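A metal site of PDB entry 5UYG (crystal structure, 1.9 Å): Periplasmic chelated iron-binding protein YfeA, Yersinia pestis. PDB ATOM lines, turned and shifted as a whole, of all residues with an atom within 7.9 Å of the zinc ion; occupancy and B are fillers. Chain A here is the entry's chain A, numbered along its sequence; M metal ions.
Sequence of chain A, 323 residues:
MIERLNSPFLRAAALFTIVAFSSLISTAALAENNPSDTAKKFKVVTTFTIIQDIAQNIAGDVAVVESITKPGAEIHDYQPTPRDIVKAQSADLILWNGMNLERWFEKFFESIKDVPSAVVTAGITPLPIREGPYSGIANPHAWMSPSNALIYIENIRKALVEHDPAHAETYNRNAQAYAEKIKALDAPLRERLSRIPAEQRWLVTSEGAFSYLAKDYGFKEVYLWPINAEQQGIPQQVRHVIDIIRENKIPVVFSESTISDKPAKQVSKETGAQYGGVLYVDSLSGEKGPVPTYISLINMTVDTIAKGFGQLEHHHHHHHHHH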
ATOM      1  N   GLU A  74      18.848   0.903   8.990  1.00  0.00           N
ATOM      2  CA  GLU A  74      18.697   1.163   7.560  1.00  0.00           C
ATOM      3  C   GLU A  74      17.377   1.907   7.316  1.00  0.00           C
ATOM      4  O   GLU A  74      16.315   1.478   7.788  1.00  0.00           O
ATOM      5  CB  GLU A  74      18.750  -0.173   6.795  1.00  0.00           C
ATOM      6  CG  GLU A  74      19.153  -0.061   5.347  1.00  0.00           C
ATOM      7  CD  GLU A  74      18.065   0.584   4.498  1.00  0.00           C
ATOM      8  OE1 GLU A  74      16.933   0.062   4.475  1.00  0.00           O
ATOM      9  OE2 GLU A  74      18.370   1.622   3.860  1.00  0.00           O
ATOM     10  N   ILE A  75      17.425   3.028   6.594  1.00  0.00           N
ATOM     11  CA  ILE A  75      16.268   3.934   6.542  1.00  0.00           C
ATOM     12  C   ILE A  75      15.406   3.779   5.276  1.00  0.00           C
ATOM     13  O   ILE A  75      14.220   4.136   5.310  1.00  0.00           O
ATOM     14  CB  ILE A  75      16.699   5.414   6.644  1.00  0.00           C
ATOM     15  CG1 ILE A  75      17.547   5.810   5.420  1.00  0.00           C
ATOM     16  CG2 ILE A  75      17.496   5.675   7.936  1.00  0.00           C
ATOM     17  CD1 ILE A  75      18.118   7.228   5.553  1.00  0.00           C
ATOM     18  N   HIS A  76      15.975   3.314   4.158  1.00  0.00           N
ATOM     19  CA  HIS A  76      15.194   3.252   2.931  1.00  0.00           C
ATOM     20  C   HIS A  76      14.032   2.281   3.061  1.00  0.00           C
ATOM     21  O   HIS A  76      12.895   2.611   2.721  1.00  0.00           O
ATOM     22  CB  HIS A  76      16.071   2.829   1.737  1.00  0.00           C
ATOM     23  CG  HIS A  76      17.177   3.783   1.417  1.00  0.00           C
ATOM     24  ND1 HIS A  76      17.211   4.530   0.258  1.00  0.00           N
ATOM     25  CD2 HIS A  76      18.300   4.094   2.102  1.00  0.00           C
ATOM     26  CE1 HIS A  76      18.310   5.252   0.238  1.00  0.00           C
ATOM     27  NE2 HIS A  76      18.994   5.014   1.350  1.00  0.00           N
ATOM     28  N   LEU A 101      13.000   8.807  -0.495  1.00  0.00           N
ATOM     29  CA  LEU A 101      13.987   8.180   0.382  1.00  0.00           C
ATOM     30  C   LEU A 101      13.330   7.105   1.240  1.00  0.00           C
ATOM     31  O   LEU A 101      13.731   5.948   1.247  1.00  0.00           O
ATOM     32  CB  LEU A 101      14.627   9.240   1.288  1.00  0.00           C
ATOM     33  CG  LEU A 101      15.497   8.673   2.425  1.00  0.00           C
ATOM     34  CD1 LEU A 101      16.736   7.948   1.881  1.00  0.00           C
ATOM     35  CD2 LEU A 101      15.908   9.733   3.447  1.00  0.00           C
ATOM     36  N   ASN A 139      17.940  10.554  -6.831  1.00  0.00           N
ATOM     37  CA  ASN A 139      18.881  10.146  -5.773  1.00  0.00           C
ATOM     38  C   ASN A 139      18.489  10.916  -4.515  1.00  0.00           C
ATOM     39  O   ASN A 139      18.571  12.145  -4.527  1.00  0.00           O
ATOM     40  CB  ASN A 139      20.334  10.468  -6.175  1.00  0.00           C
ATOM     41  CG  ASN A 139      21.358   9.950  -5.157  1.00  0.00           C
ATOM     42  OD1 ASN A 139      21.129   9.930  -3.939  1.00  0.00           O
ATOM     43  ND2 ASN A 139      22.507   9.522  -5.666  1.00  0.00           N
ATOM     44  N   PRO A 140      18.041  10.263  -3.443  1.00  0.00           N
ATOM     45  CA  PRO A 140      17.463  10.996  -2.311  1.00  0.00           C
ATOM     46  C   PRO A 140      18.463  11.643  -1.358  1.00  0.00           C
ATOM     47  O   PRO A 140      18.050  12.447  -0.510  1.00  0.00           O
ATOM     48  CB  PRO A 140      16.668   9.916  -1.576  1.00  0.00           C
ATOM     49  CG  PRO A 140      17.442   8.629  -1.842  1.00  0.00           C
ATOM     50  CD  PRO A 140      18.041   8.803  -3.234  1.00  0.00           C
ATOM     51  N   HIS A 141      19.750  11.298  -1.468  1.00  0.00           N
ATOM     52  CA  HIS A 141      20.758  11.689  -0.476  1.00  0.00           C
ATOM     53  C   HIS A 141      21.215  13.139  -0.658  1.00  0.00           C
ATOM     54  O   HIS A 141      22.419  13.417  -0.683  1.00  0.00           O
ATOM     55  CB  HIS A 141      21.960  10.734  -0.571  1.00  0.00           C
ATOM     56  CG  HIS A 141      21.608   9.282  -0.412  1.00  0.00           C
ATOM     57  ND1 HIS A 141      21.442   8.421  -1.486  1.00  0.00           N
ATOM     58  CD2 HIS A 141      21.449   8.511   0.700  1.00  0.00           C
ATOM     59  CE1 HIS A 141      21.171   7.210  -1.045  1.00  0.00           C
ATOM     60  NE2 HIS A 141      21.172   7.227   0.275  1.00  0.00           N
ATOM     61  N   TRP A 143      21.205  15.701   1.305  1.00  0.00           N
ATOM     62  CA  TRP A 143      21.812  16.350   2.449  1.00  0.00           C
ATOM     63  C   TRP A 143      23.333  16.220   2.468  1.00  0.00           C
ATOM     64  O   TRP A 143      23.973  16.893   3.279  1.00  0.00           O
ATOM     65  CB  TRP A 143      21.239  15.759   3.761  1.00  0.00           C
ATOM     66  CG  TRP A 143      21.537  14.292   3.930  1.00  0.00           C
ATOM     67  CD1 TRP A 143      22.638  13.743   4.552  1.00  0.00           C
ATOM     68  CD2 TRP A 143      20.720  13.193   3.514  1.00  0.00           C
ATOM     69  NE1 TRP A 143      22.561  12.365   4.507  1.00  0.00           N
ATOM     70  CE2 TRP A 143      21.393  11.993   3.891  1.00  0.00           C
ATOM     71  CE3 TRP A 143      19.495  13.089   2.859  1.00  0.00           C
ATOM     72  CZ2 TRP A 143      20.878  10.727   3.639  1.00  0.00           C
ATOM     73  CZ3 TRP A 143      18.973  11.829   2.611  1.00  0.00           C
ATOM     74  CH2 TRP A 143      19.677  10.658   2.995  1.00  0.00           C
ATOM     75  N   GLU A 207      26.837   1.780  -1.226  1.00  0.00           N
ATOM     76  CA  GLU A 207      25.684   2.468  -1.802  1.00  0.00           C
ATOM     77  C   GLU A 207      26.190   3.690  -2.543  1.00  0.00           C
ATOM     78  O   GLU A 207      27.163   4.328  -2.119  1.00  0.00           O
ATOM     79  CB  GLU A 207      24.672   2.880  -0.718  1.00  0.00           C
ATOM     80  CG  GLU A 207      23.353   3.437  -1.315  1.00  0.00           C
ATOM     81  CD  GLU A 207      22.363   4.020  -0.312  1.00  0.00           C
ATOM     82  OE1 GLU A 207      22.752   4.460   0.796  1.00  0.00           O
ATOM     83  OE2 GLU A 207      21.145   4.064  -0.663  1.00  0.00           O
ATOM     84  N   GLY A 208      25.549   3.992  -3.683  1.00  0.00           N
ATOM     85  CA  GLY A 208      25.850   5.218  -4.397  1.00  0.00           C
ATOM     86  C   GLY A 208      25.220   6.437  -3.736  1.00  0.00           C
ATOM     87  O   GLY A 208      24.500   7.210  -4.372  1.00  0.00           O
ATOM     88  N   ALA A 209      25.508   6.626  -2.457  1.00  0.00           N
ATOM     89  CA  ALA A 209      24.817   7.604  -1.620  1.00  0.00           C
ATOM     90  C   ALA A 209      25.498   8.969  -1.594  1.00  0.00           C
ATOM     91  O   ALA A 209      25.054   9.864  -0.866  1.00  0.00           O
ATOM     92  CB  ALA A 209      24.679   7.028  -0.203  1.00  0.00           C
ATOM     93  N   PHE A 210      26.558   9.154  -2.388  1.00  0.00           N
ATOM     94  CA  PHE A 210      27.438  10.313  -2.232  1.00  0.00           C
ATOM     95  C   PHE A 210      27.432  11.219  -3.456  1.00  0.00           C
ATOM     96  O   PHE A 210      28.274  12.118  -3.559  1.00  0.00           O
ATOM     97  CB  PHE A 210      28.855   9.822  -1.900  1.00  0.00           C
ATOM     98  CG  PHE A 210      28.901   9.039  -0.624  1.00  0.00           C
ATOM     99  CD1 PHE A 210      29.052   9.700   0.587  1.00  0.00           C
ATOM    100  CD2 PHE A 210      28.716   7.672  -0.619  1.00  0.00           C
ATOM    101  CE1 PHE A 210      29.048   9.007   1.786  1.00  0.00           C
ATOM    102  CE2 PHE A 210      28.711   6.957   0.587  1.00  0.00           C
ATOM    103  CZ  PHE A 210      28.876   7.628   1.784  1.00  0.00           C
ATOM    104  N   TRP A 225      26.205  -0.634  -5.435  1.00  0.00           N
ATOM    105  CA  TRP A 225      24.799  -0.639  -5.799  1.00  0.00           C
ATOM    106  C   TRP A 225      24.275   0.800  -5.778  1.00  0.00           C
ATOM    107  O   TRP A 225      24.702   1.594  -4.911  1.00  0.00           O
ATOM    108  CB  TRP A 225      23.928  -1.528  -4.889  1.00  0.00           C
ATOM    109  CG  TRP A 225      24.005  -1.253  -3.397  1.00  0.00           C
ATOM    110  CD1 TRP A 225      23.199  -0.420  -2.677  1.00  0.00           C
ATOM    111  CD2 TRP A 225      24.890  -1.858  -2.451  1.00  0.00           C
ATOM    112  NE1 TRP A 225      23.558  -0.443  -1.346  1.00  0.00           N
ATOM    113  CE2 TRP A 225      24.594  -1.328  -1.181  1.00  0.00           C
ATOM    114  CE3 TRP A 225      25.933  -2.798  -2.561  1.00  0.00           C
ATOM    115  CZ2 TRP A 225      25.289  -1.691  -0.031  1.00  0.00           C
ATOM    116  CZ3 TRP A 225      26.622  -3.163  -1.419  1.00  0.00           C
ATOM    117  CH2 TRP A 225      26.291  -2.612  -0.164  1.00  0.00           C
ATOM    118  N   PRO A 226      23.378   1.159  -6.685  1.00  0.00           N
ATOM    119  CA  PRO A 226      23.036   2.589  -6.846  1.00  0.00           C
ATOM    120  C   PRO A 226      22.189   3.158  -5.705  1.00  0.00           C
ATOM    121  O   PRO A 226      22.355   4.343  -5.385  1.00  0.00           O
ATOM    122  CB  PRO A 226      22.297   2.632  -8.193  1.00  0.00           C
ATOM    123  CG  PRO A 226      21.979   1.209  -8.544  1.00  0.00           C
ATOM    124  CD  PRO A 226      22.908   0.317  -7.798  1.00  0.00           C
ATOM    125  N   ILE A 227      21.301   2.380  -5.097  1.00  0.00           N
ATOM    126  CA  ILE A 227      20.500   2.814  -3.944  1.00  0.00           C
ATOM    127  C   ILE A 227      20.168   1.579  -3.119  1.00  0.00           C
ATOM    128  O   ILE A 227      20.004   0.489  -3.657  1.00  0.00           O
ATOM    129  CB  ILE A 227      19.234   3.586  -4.391  1.00  0.00           C
ATOM    130  CG1 ILE A 227      18.475   4.164  -3.194  1.00  0.00           C
ATOM    131  CG2 ILE A 227      18.276   2.682  -5.173  1.00  0.00           C
ATOM    132  CD1 ILE A 227      17.448   5.223  -3.591  1.00  0.00           C
ATOM    133  N   ASN A 228      20.072   1.758  -1.789  1.00  0.00           N
ATOM    134  CA  ASN A 228      19.747   0.622  -0.931  1.00  0.00           C
ATOM    135  C   ASN A 228      18.397   0.045  -1.331  1.00  0.00           C
ATOM    136  O   ASN A 228      17.433   0.780  -1.542  1.00  0.00           O
ATOM    137  CB  ASN A 228      19.705   1.017   0.550  1.00  0.00           C
ATOM    138  CG  ASN A 228      21.087   1.279   1.146  1.00  0.00           C
ATOM    139  OD1 ASN A 228      22.111   1.122   0.480  1.00  0.00           O
ATOM    140  ND2 ASN A 228      21.115   1.695   2.410  1.00  0.00           N
ATOM    141  N   ALA A 229      18.337  -1.290  -1.415  1.00  0.00           N
ATOM    142  CA  ALA A 229      17.125  -2.018  -1.798  1.00  0.00           C
ATOM    143  C   ALA A 229      17.441  -3.500  -1.897  1.00  0.00           C
ATOM    144  O   ALA A 229      18.584  -3.868  -2.161  1.00  0.00           O
ATOM    145  CB  ALA A 229      16.572  -1.536  -3.145  1.00  0.00           C
ATOM    146  N   GLU A 256      29.534   1.970   4.283  1.00  0.00           N
ATOM    147  CA  GLU A 256      28.714   2.952   4.999  1.00  0.00           C
ATOM    148  C   GLU A 256      28.097   2.322   6.225  1.00  0.00           C
ATOM    149  O   GLU A 256      27.964   1.099   6.319  1.00  0.00           O
ATOM    150  CB  GLU A 256      27.606   3.532   4.119  1.00  0.00           C
ATOM    151  CG  GLU A 256      28.112   4.210   2.881  1.00  0.00           C
ATOM    152  CD  GLU A 256      28.169   3.260   1.693  1.00  0.00           C
ATOM    153  OE1 GLU A 256      27.100   2.705   1.355  1.00  0.00           O
ATOM    154  OE2 GLU A 256      29.272   3.084   1.113  1.00  0.00           O
ATOM    155  N   THR A 258      25.148   2.002   7.745  1.00  0.00           N
ATOM    156  CA  THR A 258      23.919   1.235   7.943  1.00  0.00           C
ATOM    157  C   THR A 258      23.855  -0.032   7.098  1.00  0.00           C
ATOM    158  O   THR A 258      22.854  -0.743   7.164  1.00  0.00           O
ATOM    159  CB  THR A 258      22.660   2.077   7.673  1.00  0.00           C
ATOM    160  OG1 THR A 258      22.510   2.310   6.263  1.00  0.00           O
ATOM    161  CG2 THR A 258      22.692   3.403   8.447  1.00  0.00           C
ATOM    162  N   ILE A 259      24.885  -0.343   6.335  1.00  0.00           N
ATOM    163  CA  ILE A 259      24.896  -1.505   5.449  1.00  0.00           C
ATOM    164  C   ILE A 259      26.138  -2.333   5.744  1.00  0.00           C
ATOM    165  O   ILE A 259      26.986  -1.965   6.556  1.00  0.00           O
ATOM    166  CB  ILE A 259      24.818  -1.112   3.960  1.00  0.00           C
ATOM    167  CG1 ILE A 259      25.815   0.001   3.634  1.00  0.00           C
ATOM    168  CG2 ILE A 259      23.398  -0.654   3.599  1.00  0.00           C
ATOM    169  CD1 ILE A 259      27.169  -0.483   3.154  1.00  0.00           C
ATOM    170  N   VAL A 281      26.333   8.444   6.093  1.00  0.00           N
ATOM    171  CA  VAL A 281      25.444   9.190   5.192  1.00  0.00           C
ATOM    172  C   VAL A 281      23.991   9.009   5.622  1.00  0.00           C
ATOM    173  O   VAL A 281      23.251   9.994   5.768  1.00  0.00           O
ATOM    174  CB  VAL A 281      25.645   8.751   3.722  1.00  0.00           C
ATOM    175  CG1 VAL A 281      25.635   7.217   3.582  1.00  0.00           C
ATOM    176  CG2 VAL A 281      24.572   9.371   2.812  1.00  0.00           C
ATOM    177  N   ASP A 282      23.549   7.777   5.838  1.00  0.00           N
ATOM    178  CA  ASP A 282      22.128   7.542   6.106  1.00  0.00           C
ATOM    179  C   ASP A 282      21.770   7.638   7.578  1.00  0.00           C
ATOM    180  O   ASP A 282      20.578   7.668   7.912  1.00  0.00           O
ATOM    181  CB  ASP A 282      21.688   6.157   5.592  1.00  0.00           C
ATOM    182  CG  ASP A 282      21.512   6.136   4.087  1.00  0.00           C
ATOM    183  OD1 ASP A 282      21.632   7.198   3.427  1.00  0.00           O
ATOM    184  OD2 ASP A 282      21.224   5.029   3.567  1.00  0.00           O
ATOM    185  N   SER A 283      22.750   7.723   8.478  1.00  0.00           N
ATOM    186  CA  SER A 283      22.418   7.803   9.892  1.00  0.00           C
ATOM    187  C   SER A 283      23.554   8.451  10.647  1.00  0.00           C
ATOM    188  O   SER A 283      24.723   8.330  10.264  1.00  0.00           O
ATOM    189  CB  SER A 283      22.122   6.413  10.472  1.00  0.00           C
ATOM    190  OG  SER A 283      21.930   6.492  11.873  1.00  0.00           O
HETATM  191 ZN    ZN M   1      21.035   5.489   1.464  1.00  0.00          ZN
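N of His 76 lies within hydrogen-bond range of OE2 of Glu 74, at 2.9 Å. The backbone NH of Asn 228 sits close to the side-chain carboxylate of Glu 207 (2.8 Å). OE1 of Glu 256 sits at hydrogen-bond distance from N of Glu 207. The side-chain amide oxygen (OD1) of Asn 139 sits at hydrogen-bond distance from a ring nitrogen (ND1) of His 141, 2.9 Å away. The side-chain amide nitrogen of Asn 228 is in hydrogen-bond range of the side-chain carboxylate of Glu 74 (3.1 Å). The side-chain amide oxygen (OD1) of Asn 228 sits at hydrogen-bond distance from the indole nitrogen (NE1) of Trp 225 (2.8 Å).
Asn 228 touches the zinc ion. Five residues have an atom within 4 Å of the zinc ion: His 76, His 141, Glu 207, Asn 228 and Asp 282. The nearest printed residue that does not touch the zinc ion is Ala 209 (4.3 Å).
The zinc ion is bound by NE2 of His 76 (2.1 Å), OE1 of Glu 207 (2.1 Å), NE2 of His 141 (2.1 Å), OD2 of Asp 282 (2.2 Å) and OE2 of Glu 207 (2.6 Å). The zinc ion has five donor atoms within binding distance. Slightly farther from the zinc ion lies the side-chain carboxylate (OD1) of Asp 282 (2.7 Å).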
